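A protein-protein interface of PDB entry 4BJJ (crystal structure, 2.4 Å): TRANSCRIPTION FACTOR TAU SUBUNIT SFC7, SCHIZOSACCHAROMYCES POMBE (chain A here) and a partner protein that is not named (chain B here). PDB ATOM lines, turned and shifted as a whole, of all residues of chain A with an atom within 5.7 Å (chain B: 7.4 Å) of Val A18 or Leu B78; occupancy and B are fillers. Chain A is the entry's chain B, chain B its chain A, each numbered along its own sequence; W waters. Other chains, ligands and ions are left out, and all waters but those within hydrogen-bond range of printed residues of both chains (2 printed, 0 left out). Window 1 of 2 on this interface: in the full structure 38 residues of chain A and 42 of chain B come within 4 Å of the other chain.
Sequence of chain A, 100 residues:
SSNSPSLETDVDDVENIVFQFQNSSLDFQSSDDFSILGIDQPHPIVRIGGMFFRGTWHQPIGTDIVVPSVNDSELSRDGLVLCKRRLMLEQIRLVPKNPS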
ATOM      1  N   ASN A  16     -10.549  15.356 -18.473  1.00  0.00           N
ATOM      2  CA  ASN A  16      -9.213  15.640 -19.032  1.00  0.00           C
ATOM      3  C   ASN A  16      -8.755  14.642 -20.083  1.00  0.00           C
ATOM      4  O   ASN A  16      -8.755  13.443 -19.847  1.00  0.00           O
ATOM      5  CB  ASN A  16      -8.161  15.685 -17.930  1.00  0.00           C
ATOM      6  CG  ASN A  16      -8.284  16.916 -17.062  1.00  0.00           C
ATOM      7  OD1 ASN A  16      -7.919  18.023 -17.482  1.00  0.00           O
ATOM      8  ND2 ASN A  16      -8.802  16.737 -15.844  1.00  0.00           N
ATOM      9  N   ILE A  17      -8.336  15.159 -21.230  1.00  0.00           N
ATOM     10  CA  ILE A  17      -8.068  14.335 -22.392  1.00  0.00           C
ATOM     11  C   ILE A  17      -6.699  14.621 -22.962  1.00  0.00           C
ATOM     12  O   ILE A  17      -6.319  15.772 -23.164  1.00  0.00           O
ATOM     13  CB  ILE A  17      -9.140  14.565 -23.522  1.00  0.00           C
ATOM     14  CG1 ILE A  17     -10.562  14.366 -22.975  1.00  0.00           C
ATOM     15  CG2 ILE A  17      -8.912  13.608 -24.684  1.00  0.00           C
ATOM     16  CD1 ILE A  17     -11.631  14.822 -23.918  1.00  0.00           C
ATOM     17  N   VAL A  18      -5.947  13.564 -23.221  1.00  0.00           N
ATOM     18  CA  VAL A  18      -4.664  13.725 -23.897  1.00  0.00           C
ATOM     19  C   VAL A  18      -4.855  13.820 -25.416  1.00  0.00           C
ATOM     20  O   VAL A  18      -5.601  13.033 -26.000  1.00  0.00           O
ATOM     21  CB  VAL A  18      -3.744  12.560 -23.559  1.00  0.00           C
ATOM     22  CG1 VAL A  18      -2.452  12.678 -24.316  1.00  0.00           C
ATOM     23  CG2 VAL A  18      -3.501  12.535 -22.061  1.00  0.00           C
ATOM     24  N   PHE A  19      -4.212  14.815 -26.023  1.00  0.00           N
ATOM     25  CA  PHE A  19      -4.149  14.955 -27.474  1.00  0.00           C
ATOM     26  C   PHE A  19      -2.756  14.578 -27.969  1.00  0.00           C
ATOM     27  O   PHE A  19      -1.745  15.182 -27.562  1.00  0.00           O
ATOM     28  CB  PHE A  19      -4.451  16.393 -27.903  1.00  0.00           C
ATOM     29  CG  PHE A  19      -5.923  16.758 -27.899  1.00  0.00           C
ATOM     30  CD1 PHE A  19      -6.827  16.106 -27.087  1.00  0.00           C
ATOM     31  CD2 PHE A  19      -6.395  17.775 -28.716  1.00  0.00           C
ATOM     32  CE1 PHE A  19      -8.184  16.457 -27.091  1.00  0.00           C
ATOM     33  CE2 PHE A  19      -7.756  18.131 -28.729  1.00  0.00           C
ATOM     34  CZ  PHE A  19      -8.640  17.472 -27.905  1.00  0.00           C
ATOM     35  N   GLN A  20      -2.692  13.566 -28.825  1.00  0.00           N
ATOM     36  CA  GLN A  20      -1.424  13.125 -29.372  1.00  0.00           C
ATOM     37  C   GLN A  20      -1.388  13.287 -30.897  1.00  0.00           C
ATOM     38  O   GLN A  20      -2.345  13.014 -31.599  1.00  0.00           O
ATOM     39  CB  GLN A  20      -1.150  11.684 -28.989  1.00  0.00           C
ATOM     40  CG  GLN A  20       0.193  11.219 -29.464  1.00  0.00           C
ATOM     41  CD  GLN A  20       0.416   9.771 -29.204  1.00  0.00           C
ATOM     42  OE1 GLN A  20      -0.372   9.126 -28.503  1.00  0.00           O
ATOM     43  NE2 GLN A  20       1.516   9.234 -29.753  1.00  0.00           N
ATOM     44  N   PHE A  21      -0.247  13.716 -31.404  1.00  0.00           N
ATOM     45  CA  PHE A  21      -0.159  14.152 -32.767  1.00  0.00           C
ATOM     46  C   PHE A  21       0.684  13.185 -33.559  1.00  0.00           C
ATOM     47  O   PHE A  21       1.712  12.741 -33.106  1.00  0.00           O
ATOM     48  CB  PHE A  21       0.410  15.557 -32.806  1.00  0.00           C
ATOM     49  CG  PHE A  21      -0.529  16.585 -32.274  1.00  0.00           C
ATOM     50  CD1 PHE A  21      -0.533  16.909 -30.934  1.00  0.00           C
ATOM     51  CD2 PHE A  21      -1.429  17.221 -33.115  1.00  0.00           C
ATOM     52  CE1 PHE A  21      -1.417  17.853 -30.423  1.00  0.00           C
ATOM     53  CE2 PHE A  21      -2.315  18.164 -32.626  1.00  0.00           C
ATOM     54  CZ  PHE A  21      -2.311  18.485 -31.277  1.00  0.00           C
ATOM     55  N   PHE A  28       3.461  23.620 -30.947  1.00  0.00           N
ATOM     56  CA  PHE A  28       2.306  24.291 -30.357  1.00  0.00           C
ATOM     57  C   PHE A  28       2.773  24.912 -29.059  1.00  0.00           C
ATOM     58  O   PHE A  28       3.159  24.210 -28.129  1.00  0.00           O
ATOM     59  CB  PHE A  28       1.136  23.323 -30.074  1.00  0.00           C
ATOM     60  CG  PHE A  28       0.860  22.339 -31.187  1.00  0.00           C
ATOM     61  CD1 PHE A  28       0.536  22.772 -32.461  1.00  0.00           C
ATOM     62  CD2 PHE A  28       0.919  20.983 -30.950  1.00  0.00           C
ATOM     63  CE1 PHE A  28       0.295  21.875 -33.471  1.00  0.00           C
ATOM     64  CE2 PHE A  28       0.665  20.081 -31.954  1.00  0.00           C
ATOM     65  CZ  PHE A  28       0.357  20.526 -33.222  1.00  0.00           C
ATOM     66  N   PHE A  34      -6.580  28.019 -30.076  1.00  0.00           N
ATOM     67  CA  PHE A  34      -7.023  26.649 -30.013  1.00  0.00           C
ATOM     68  C   PHE A  34      -8.550  26.573 -30.074  1.00  0.00           C
ATOM     69  O   PHE A  34      -9.242  27.255 -29.328  1.00  0.00           O
ATOM     70  CB  PHE A  34      -6.564  26.047 -28.692  1.00  0.00           C
ATOM     71  CG  PHE A  34      -6.900  24.592 -28.542  1.00  0.00           C
ATOM     72  CD1 PHE A  34      -8.120  24.192 -28.043  1.00  0.00           C
ATOM     73  CD2 PHE A  34      -5.974  23.619 -28.893  1.00  0.00           C
ATOM     74  CE1 PHE A  34      -8.411  22.843 -27.898  1.00  0.00           C
ATOM     75  CE2 PHE A  34      -6.260  22.264 -28.747  1.00  0.00           C
ATOM     76  CZ  PHE A  34      -7.468  21.871 -28.242  1.00  0.00           C
ATOM     77  N   ILE A  48      -5.328  24.688 -34.458  1.00  0.00           N
ATOM     78  CA  ILE A  48      -4.319  25.255 -33.586  1.00  0.00           C
ATOM     79  C   ILE A  48      -3.446  26.177 -34.414  1.00  0.00           C
ATOM     80  O   ILE A  48      -2.831  25.742 -35.369  1.00  0.00           O
ATOM     81  CB  ILE A  48      -3.431  24.165 -32.932  1.00  0.00           C
ATOM     82  CG1 ILE A  48      -4.301  23.099 -32.269  1.00  0.00           C
ATOM     83  CG2 ILE A  48      -2.532  24.797 -31.890  1.00  0.00           C
ATOM     84  CD1 ILE A  48      -3.557  21.863 -31.866  1.00  0.00           C
ATOM     85  N   ASP A  64      -2.873   6.410 -18.057  1.00  0.00           N
ATOM     86  CA  ASP A  64      -2.001   7.574 -18.065  1.00  0.00           C
ATOM     87  C   ASP A  64      -1.975   8.215 -16.692  1.00  0.00           C
ATOM     88  O   ASP A  64      -3.009   8.333 -16.030  1.00  0.00           O
ATOM     89  CB  ASP A  64      -2.485   8.589 -19.103  1.00  0.00           C
ATOM     90  CG  ASP A  64      -2.137   8.179 -20.525  1.00  0.00           C
ATOM     91  OD1 ASP A  64      -1.652   7.039 -20.712  1.00  0.00           O
ATOM     92  OD2 ASP A  64      -2.350   8.985 -21.460  1.00  0.00           O
ATOM     93  N   VAL A  66      -0.851  11.889 -15.212  1.00  0.00           N
ATOM     94  CA  VAL A  66      -0.464  13.237 -15.600  1.00  0.00           C
ATOM     95  C   VAL A  66      -0.124  14.010 -14.341  1.00  0.00           C
ATOM     96  O   VAL A  66      -0.931  14.137 -13.429  1.00  0.00           O
ATOM     97  CB  VAL A  66      -1.573  13.929 -16.432  1.00  0.00           C
ATOM     98  CG1 VAL A  66      -0.981  15.015 -17.266  1.00  0.00           C
ATOM     99  CG2 VAL A  66      -2.242  12.914 -17.354  1.00  0.00           C
ATOM    100  N   LEU A  82      -5.693   8.974 -15.743  1.00  0.00           N
ATOM    101  CA  LEU A  82      -6.641   8.885 -16.854  1.00  0.00           C
ATOM    102  C   LEU A  82      -6.656   7.496 -17.451  1.00  0.00           C
ATOM    103  O   LEU A  82      -5.630   6.998 -17.926  1.00  0.00           O
ATOM    104  CB  LEU A  82      -6.281   9.885 -17.936  1.00  0.00           C
ATOM    105  CG  LEU A  82      -6.065  11.312 -17.440  1.00  0.00           C
ATOM    106  CD1 LEU A  82      -5.640  12.196 -18.594  1.00  0.00           C
ATOM    107  CD2 LEU A  82      -7.324  11.842 -16.783  1.00  0.00           C
ATOM    108  N   ARG A  85     -10.171   7.398 -23.211  1.00  0.00           N
ATOM    109  CA  ARG A  85      -9.587   7.528 -24.543  1.00  0.00           C
ATOM    110  C   ARG A  85      -8.703   8.774 -24.761  1.00  0.00           C
ATOM    111  O   ARG A  85      -8.867   9.788 -24.113  1.00  0.00           O
ATOM    112  CB  ARG A  85     -10.690   7.471 -25.600  1.00  0.00           C
ATOM    113  CG  ARG A  85     -11.319   6.089 -25.762  1.00  0.00           C
ATOM    114  CD  ARG A  85     -12.324   6.028 -26.921  1.00  0.00           C
ATOM    115  NE  ARG A  85     -13.349   7.068 -26.835  1.00  0.00           N
ATOM    116  CZ  ARG A  85     -14.288   7.266 -27.761  1.00  0.00           C
ATOM    117  NH1 ARG A  85     -14.323   6.488 -28.840  1.00  0.00           N
ATOM    118  NH2 ARG A  85     -15.191   8.237 -27.614  1.00  0.00           N
ATOM    119  N   ARG A  86      -7.754   8.682 -25.682  1.00  0.00           N
ATOM    120  CA  ARG A  86      -7.070   9.880 -26.136  1.00  0.00           C
ATOM    121  C   ARG A  86      -7.376  10.121 -27.596  1.00  0.00           C
ATOM    122  O   ARG A  86      -7.790   9.214 -28.326  1.00  0.00           O
ATOM    123  CB  ARG A  86      -5.562   9.814 -25.900  1.00  0.00           C
ATOM    124  CG  ARG A  86      -4.890   8.699 -26.584  1.00  0.00           C
ATOM    125  CD  ARG A  86      -3.407   8.836 -26.525  1.00  0.00           C
ATOM    126  NE  ARG A  86      -2.891   8.641 -25.179  1.00  0.00           N
ATOM    127  CZ  ARG A  86      -1.594   8.671 -24.879  1.00  0.00           C
ATOM    128  NH1 ARG A  86      -0.679   8.886 -25.830  1.00  0.00           N
ATOM    129  NH2 ARG A  86      -1.216   8.482 -23.627  1.00  0.00           N
ATOM    130  N   LEU A  87      -7.171  11.366 -28.002  1.00  0.00           N
ATOM    131  CA  LEU A  87      -7.416  11.778 -29.358  1.00  0.00           C
ATOM    132  C   LEU A  87      -6.124  11.816 -30.139  1.00  0.00           C
ATOM    133  O   LEU A  87      -5.182  12.482 -29.750  1.00  0.00           O
ATOM    134  CB  LEU A  87      -8.058  13.162 -29.372  1.00  0.00           C
ATOM    135  CG  LEU A  87      -8.642  13.525 -30.735  1.00  0.00           C
ATOM    136  CD1 LEU A  87      -9.876  12.675 -30.995  1.00  0.00           C
ATOM    137  CD2 LEU A  87      -8.955  15.005 -30.811  1.00  0.00           C
ATOM    138  N   MET A  88      -6.128  11.120 -31.267  1.00  0.00           N
ATOM    139  CA  MET A  88      -4.991  11.019 -32.166  1.00  0.00           C
ATOM    140  C   MET A  88      -5.212  11.921 -33.362  1.00  0.00           C
ATOM    141  O   MET A  88      -6.150  11.708 -34.115  1.00  0.00           O
ATOM    142  CB  MET A  88      -4.884   9.573 -32.665  1.00  0.00           C
ATOM    143  CG  MET A  88      -4.915   8.525 -31.556  1.00  0.00           C
ATOM    144  SD  MET A  88      -3.566   8.686 -30.351  1.00  0.00           S
ATOM    145  CE  MET A  88      -2.340   7.716 -31.204  1.00  0.00           C
ATOM    146  N   ILE B   8      -3.814  28.455 -25.727  1.00  0.00           N
ATOM    147  CA  ILE B   8      -3.096  27.456 -24.911  1.00  0.00           C
ATOM    148  C   ILE B   8      -2.403  28.140 -23.738  1.00  0.00           C
ATOM    149  O   ILE B   8      -1.636  29.090 -23.921  1.00  0.00           O
ATOM    150  CB  ILE B   8      -2.020  26.672 -25.728  1.00  0.00           C
ATOM    151  CG1 ILE B   8      -2.660  25.888 -26.854  1.00  0.00           C
ATOM    152  CG2 ILE B   8      -1.217  25.693 -24.830  1.00  0.00           C
ATOM    153  CD1 ILE B   8      -1.648  25.260 -27.803  1.00  0.00           C
ATOM    154  N   TYR B  13       2.835  19.806 -17.866  1.00  0.00           N
ATOM    155  CA  TYR B  13       2.728  18.527 -17.178  1.00  0.00           C
ATOM    156  C   TYR B  13       3.740  17.527 -17.695  1.00  0.00           C
ATOM    157  O   TYR B  13       4.245  17.665 -18.809  1.00  0.00           O
ATOM    158  CB  TYR B  13       1.355  17.909 -17.398  1.00  0.00           C
ATOM    159  CG  TYR B  13       0.219  18.693 -16.833  1.00  0.00           C
ATOM    160  CD1 TYR B  13      -0.270  19.813 -17.482  1.00  0.00           C
ATOM    161  CD2 TYR B  13      -0.377  18.303 -15.656  1.00  0.00           C
ATOM    162  CE1 TYR B  13      -1.317  20.526 -16.951  1.00  0.00           C
ATOM    163  CE2 TYR B  13      -1.409  18.978 -15.139  1.00  0.00           C
ATOM    164  CZ  TYR B  13      -1.889  20.087 -15.778  1.00  0.00           C
ATOM    165  OH  TYR B  13      -2.948  20.755 -15.209  1.00  0.00           O
ATOM    166  N   LEU B  15       3.918  13.228 -18.386  1.00  0.00           N
ATOM    167  CA  LEU B  15       2.953  12.165 -18.634  1.00  0.00           C
ATOM    168  C   LEU B  15       3.646  10.837 -18.501  1.00  0.00           C
ATOM    169  O   LEU B  15       4.687  10.630 -19.075  1.00  0.00           O
ATOM    170  CB  LEU B  15       2.352  12.317 -20.027  1.00  0.00           C
ATOM    171  CG  LEU B  15       1.544  11.136 -20.577  1.00  0.00           C
ATOM    172  CD1 LEU B  15       0.245  10.999 -19.812  1.00  0.00           C
ATOM    173  CD2 LEU B  15       1.301  11.311 -22.075  1.00  0.00           C
ATOM    174  N   GLU B  17       3.098   6.972 -19.291  1.00  0.00           N
ATOM    175  CA  GLU B  17       2.283   5.981 -20.002  1.00  0.00           C
ATOM    176  C   GLU B  17       2.494   4.596 -19.416  1.00  0.00           C
ATOM    177  O   GLU B  17       3.363   3.849 -19.850  1.00  0.00           O
ATOM    178  CB  GLU B  17       2.572   6.020 -21.506  1.00  0.00           C
ATOM    179  CG  GLU B  17       2.137   7.331 -22.169  1.00  0.00           C
ATOM    180  CD  GLU B  17       2.216   7.309 -23.705  1.00  0.00           C
ATOM    181  OE1 GLU B  17       2.609   6.274 -24.310  1.00  0.00           O
ATOM    182  OE2 GLU B  17       1.884   8.346 -24.314  1.00  0.00           O
ATOM    183  N   ARG B  75       7.222  15.002 -26.922  1.00  0.00           N
ATOM    184  CA  ARG B  75       6.475  15.073 -28.168  1.00  0.00           C
ATOM    185  C   ARG B  75       5.845  16.429 -28.112  1.00  0.00           C
ATOM    186  O   ARG B  75       6.439  17.344 -27.561  1.00  0.00           O
ATOM    187  CB  ARG B  75       5.443  13.943 -28.271  1.00  0.00           C
ATOM    188  CG  ARG B  75       6.118  12.584 -28.198  1.00  0.00           C
ATOM    189  CD  ARG B  75       5.205  11.424 -28.436  1.00  0.00           C
ATOM    190  NE  ARG B  75       4.224  11.279 -27.380  1.00  0.00           N
ATOM    191  CZ  ARG B  75       3.777  10.115 -26.926  1.00  0.00           C
ATOM    192  NH1 ARG B  75       4.240   8.970 -27.411  1.00  0.00           N
ATOM    193  NH2 ARG B  75       2.897  10.101 -25.944  1.00  0.00           N
ATOM    194  N   ASN B  76       4.653  16.573 -28.681  1.00  0.00           N
ATOM    195  CA  ASN B  76       3.928  17.818 -28.605  1.00  0.00           C
ATOM    196  C   ASN B  76       2.528  17.568 -28.098  1.00  0.00           C
ATOM    197  O   ASN B  76       1.563  18.183 -28.551  1.00  0.00           O
ATOM    198  CB  ASN B  76       3.912  18.490 -29.971  1.00  0.00           C
ATOM    199  CG  ASN B  76       3.459  17.562 -31.086  1.00  0.00           C
ATOM    200  OD1 ASN B  76       3.173  16.383 -30.882  1.00  0.00           O
ATOM    201  ND2 ASN B  76       3.387  18.110 -32.280  1.00  0.00           N
ATOM    202  N   ASP B  77       2.421  16.670 -27.129  1.00  0.00           N
ATOM    203  CA  ASP B  77       1.121  16.288 -26.624  1.00  0.00           C
ATOM    204  C   ASP B  77       0.515  17.432 -25.822  1.00  0.00           C
ATOM    205  O   ASP B  77       1.222  18.247 -25.213  1.00  0.00           O
ATOM    206  CB  ASP B  77       1.222  15.046 -25.742  1.00  0.00           C
ATOM    207  CG  ASP B  77       2.013  13.915 -26.391  1.00  0.00           C
ATOM    208  OD1 ASP B  77       1.704  13.570 -27.545  1.00  0.00           O
ATOM    209  OD2 ASP B  77       2.943  13.370 -25.747  1.00  0.00           O
ATOM    210  N   LEU B  78      -0.809  17.466 -25.803  1.00  0.00           N
ATOM    211  CA  LEU B  78      -1.522  18.482 -25.071  1.00  0.00           C
ATOM    212  C   LEU B  78      -2.474  17.817 -24.130  1.00  0.00           C
ATOM    213  O   LEU B  78      -2.931  16.709 -24.374  1.00  0.00           O
ATOM    214  CB  LEU B  78      -2.292  19.412 -26.018  1.00  0.00           C
ATOM    215  CG  LEU B  78      -1.449  20.108 -27.092  1.00  0.00           C
ATOM    216  CD1 LEU B  78      -2.370  20.833 -28.059  1.00  0.00           C
ATOM    217  CD2 LEU B  78      -0.497  21.102 -26.476  1.00  0.00           C
ATOM    218  N   LEU B  79      -2.757  18.504 -23.041  1.00  0.00           N
ATOM    219  CA  LEU B  79      -3.734  18.052 -22.096  1.00  0.00           C
ATOM    220  C   LEU B  79      -4.925  19.008 -22.192  1.00  0.00           C
ATOM    221  O   LEU B  79      -4.781  20.208 -22.005  1.00  0.00           O
ATOM    222  CB  LEU B  79      -3.164  18.052 -20.690  1.00  0.00           C
ATOM    223  CG  LEU B  79      -4.175  17.570 -19.660  1.00  0.00           C
ATOM    224  CD1 LEU B  79      -4.484  16.076 -19.830  1.00  0.00           C
ATOM    225  CD2 LEU B  79      -3.673  17.873 -18.292  1.00  0.00           C
ATOM    226  N   VAL B  80      -6.095  18.458 -22.477  1.00  0.00           N
ATOM    227  CA  VAL B  80      -7.254  19.274 -22.791  1.00  0.00           C
ATOM    228  C   VAL B  80      -8.335  19.028 -21.768  1.00  0.00           C
ATOM    229  O   VAL B  80      -8.831  17.908 -21.610  1.00  0.00           O
ATOM    230  CB  VAL B  80      -7.775  18.959 -24.199  1.00  0.00           C
ATOM    231  CG1 VAL B  80      -8.998  19.795 -24.520  1.00  0.00           C
ATOM    232  CG2 VAL B  80      -6.684  19.211 -25.229  1.00  0.00           C
ATOM    233  N   THR B  81      -8.679  20.092 -21.055  1.00  0.00           N
ATOM    234  CA  THR B  81      -9.694  20.032 -20.021  1.00  0.00           C
ATOM    235  C   THR B  81     -11.015  20.552 -20.587  1.00  0.00           C
ATOM    236  O   THR B  81     -11.084  21.689 -21.051  1.00  0.00           O
ATOM    237  CB  THR B  81      -9.275  20.883 -18.807  1.00  0.00           C
ATOM    238  OG1 THR B  81      -7.975  20.475 -18.355  1.00  0.00           O
ATOM    239  CG2 THR B  81     -10.271  20.739 -17.672  1.00  0.00           C
ATOM    240  N   VAL B  92      -6.260  24.259 -22.084  1.00  0.00           N
ATOM    241  CA  VAL B  92      -5.294  23.450 -22.822  1.00  0.00           C
ATOM    242  C   VAL B  92      -3.897  23.684 -22.263  1.00  0.00           C
ATOM    243  O   VAL B  92      -3.487  24.817 -22.111  1.00  0.00           O
ATOM    244  CB  VAL B  92      -5.284  23.768 -24.331  1.00  0.00           C
ATOM    245  CG1 VAL B  92      -4.349  22.809 -25.073  1.00  0.00           C
ATOM    246  CG2 VAL B  92      -6.697  23.706 -24.913  1.00  0.00           C
ATOM    247  N   SER B  93      -3.168  22.601 -21.988  1.00  0.00           N
ATOM    248  CA  SER B  93      -1.820  22.670 -21.415  1.00  0.00           C
ATOM    249  C   SER B  93      -0.858  21.733 -22.143  1.00  0.00           C
ATOM    250  O   SER B  93      -1.263  20.710 -22.672  1.00  0.00           O
ATOM    251  CB  SER B  93      -1.847  22.286 -19.934  1.00  0.00           C
ATOM    252  OG  SER B  93      -2.825  23.016 -19.244  1.00  0.00           O
ATOM    253  N   ARG B  94       0.420  22.085 -22.154  1.00  0.00           N
ATOM    254  CA  ARG B  94       1.409  21.236 -22.793  1.00  0.00           C
ATOM    255  C   ARG B  94       1.916  20.133 -21.852  1.00  0.00           C
ATOM    256  O   ARG B  94       2.117  20.344 -20.675  1.00  0.00           O
ATOM    257  CB  ARG B  94       2.571  22.066 -23.308  1.00  0.00           C
ATOM    258  CG  ARG B  94       2.156  23.095 -24.316  1.00  0.00           C
ATOM    259  CD  ARG B  94       3.356  23.849 -24.866  1.00  0.00           C
ATOM    260  NE  ARG B  94       4.347  22.964 -25.476  1.00  0.00           N
ATOM    261  CZ  ARG B  94       5.566  23.345 -25.873  1.00  0.00           C
ATOM    262  NH1 ARG B  94       5.949  24.601 -25.708  1.00  0.00           N
ATOM    263  NH2 ARG B  94       6.407  22.469 -26.438  1.00  0.00           N
ATOM    264  N   ILE B  95       2.044  18.937 -22.404  1.00  0.00           N
ATOM    265  CA  ILE B  95       2.703  17.832 -21.769  1.00  0.00           C
ATOM    266  C   ILE B  95       4.151  17.914 -22.314  1.00  0.00           C
ATOM    267  O   ILE B  95       4.401  17.646 -23.492  1.00  0.00           O
ATOM    268  CB  ILE B  95       2.003  16.509 -22.157  1.00  0.00           C
ATOM    269  CG1 ILE B  95       0.567  16.500 -21.642  1.00  0.00           C
ATOM    270  CG2 ILE B  95       2.735  15.299 -21.617  1.00  0.00           C
ATOM    271  CD1 ILE B  95      -0.306  15.371 -22.225  1.00  0.00           C
ATOM    272  N   ARG B  96       5.095  18.315 -21.465  1.00  0.00           N
ATOM    273  CA  ARG B  96       6.457  18.604 -21.925  1.00  0.00           C
ATOM    274  C   ARG B  96       7.337  17.367 -21.979  1.00  0.00           C
ATOM    275  O   ARG B  96       8.271  17.329 -22.765  1.00  0.00           O
ATOM    276  CB  ARG B  96       7.129  19.673 -21.063  1.00  0.00           C
ATOM    277  CG  ARG B  96       6.502  21.062 -21.129  1.00  0.00           C
ATOM    278  CD  ARG B  96       6.281  21.578 -22.523  1.00  0.00           C
ATOM    279  NE  ARG B  96       7.490  21.723 -23.327  1.00  0.00           N
ATOM    280  CZ  ARG B  96       8.262  22.814 -23.336  1.00  0.00           C
ATOM    281  NH1 ARG B  96       7.988  23.845 -22.558  1.00  0.00           N
ATOM    282  NH2 ARG B  96       9.337  22.856 -24.097  1.00  0.00           N
ATOM    283  N   ARG B 102       4.448   1.794 -22.124  1.00  0.00           N
ATOM    284  CA  ARG B 102       3.721   1.007 -23.138  1.00  0.00           C
ATOM    285  C   ARG B 102       4.547   0.896 -24.390  1.00  0.00           C
ATOM    286  O   ARG B 102       5.342   1.784 -24.688  1.00  0.00           O
ATOM    287  CB  ARG B 102       2.383   1.642 -23.496  1.00  0.00           C
ATOM    288  CG  ARG B 102       1.540   1.904 -22.296  1.00  0.00           C
ATOM    289  CD  ARG B 102       0.116   2.139 -22.649  1.00  0.00           C
ATOM    290  NE  ARG B 102      -0.134   3.516 -23.026  1.00  0.00           N
ATOM    291  CZ  ARG B 102      -0.571   4.467 -22.203  1.00  0.00           C
ATOM    292  NH1 ARG B 102      -0.789   4.217 -20.914  1.00  0.00           N
ATOM    293  NH2 ARG B 102      -0.797   5.682 -22.686  1.00  0.00           N
HETATM  294  O   HOH W   1       2.183  14.167 -29.885  1.00  0.00           O
HETATM  295  O   HOH W   2       3.450  21.164 -28.016  1.00  0.00           O
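The backbone carbonyl oxygen (O) of Tyr B13 lies within hydrogen-bond range of the backbone NH (N) of Arg B96, at 2.9 Å.
OE2 of Glu B17 is in salt-bridge range of NH2 of Arg B75.
The backbone NH (N) of Leu B79 lies within hydrogen-bond range of the backbone carbonyl oxygen (O) of Ser B93, 2.7 Å away.
The backbone carbonyl oxygen (O) of Val A18 is in hydrogen-bond range of the backbone NH (N) of Leu A87, 3.0 Å away.
The side-chain amide oxygen of Gln A20 lies close to the side-chain sulfur of Met A88 (3.7 Å).
The guanidinium group of Arg A86 lies within salt-bridge range of the side-chain carboxylate of Asp A64 (2.5 Å).
The side-chain carboxylate (OE2) of Glu B17 is in salt-bridge range of the guanidinium group (NH1) of Arg A86 (3.0 Å).
The backbone carbonyl oxygen (O) of Leu B78 lies within hydrogen-bond range of the backbone NH (N) of Phe A19 (2.8 Å).
The backbone NH (N) of Val B80 lies within hydrogen-bond range of the backbone carbonyl oxygen (O) of Ile A17, 2.8 Å away.
OG1 of Thr B81 lies within hydrogen-bond range of OD1 of Asn A16 (2.6 Å).
The guanidinium group (NE) of Arg B94 lies within hydrogen-bond range of the backbone carbonyl oxygen (O) of Phe A28 (3.2 Å).
OD1 of Asp A64 lies within salt-bridge range of NH2 of Arg B102 (2.5 Å).
The guanidinium group of Arg A86 sits close to the guanidinium group of Arg B102.
Water W1 lies within hydrogen-bond range of OD1 of Asp B77 (2.5 Å), OD1 of Asn B76 (2.6 Å) and N of Phe A21 (2.9 Å).
Water W2 bridges the backbone carbonyl oxygen (O) of Phe A28 (3.1 Å) and the guanidinium group (NE) of Arg B94 (3.2 Å).
Of chain A, only Ile A17 (3.7 Å), Val A18 (3.5 Å), Phe A19 (2.8 Å) and Phe A21 (3.9 Å) come within 4 Å of Leu B78.
Printed residues of chain A within 4 Å of Tyr B13: Val A66 (3.7 Å).
Of the printed residues of chain A, Thr B81 touches Asn A16.
Of the printed residues of chain A, Asn B76 touches Phe A21 (3.4 Å) and Phe A28 (3.4 Å).
Printed residues of chain B within 4 Å of Ile A17: Leu B78, Leu B79 and Val B80.
The nearest residue of chain B that does not touch Val A18 is Ile B95 (4.03 Å).
The nearest residue of chain A that does not touch Leu B78 is Ile A48 (4.1 Å).
The nearest printed residue of chain B that does not touch Asp A64 is Glu B17 (4.1 Å).
Among the printed residues, pairs that only touch across the chains: Asn A16 with Val B80, Ile A17 with Leu B78, Ile A17 with Leu B79, Val A18 with Leu B78, Phe A19 with Asp B77, Phe A19 with Val B80, Gln A20 with Arg B75, Gln A20 with Asp B77, Phe A21 with Asn B76, Phe A21 with Leu B78, Phe A28 with Asn B76, Phe A34 with Val B92, Asp A64 with Leu B15, Val A66 with Tyr B13, Val A66 with Leu B15 and Arg A86 with Arg B75.
Of the 17 printed residues of chain B, 13 touch a printed residue of chain A.
Hydrophobic or aromatic side chains of chain A that line the printed part of chain B: Ile A17, Phe A19, Phe A21, Phe A28, Phe A34 and Val A66.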
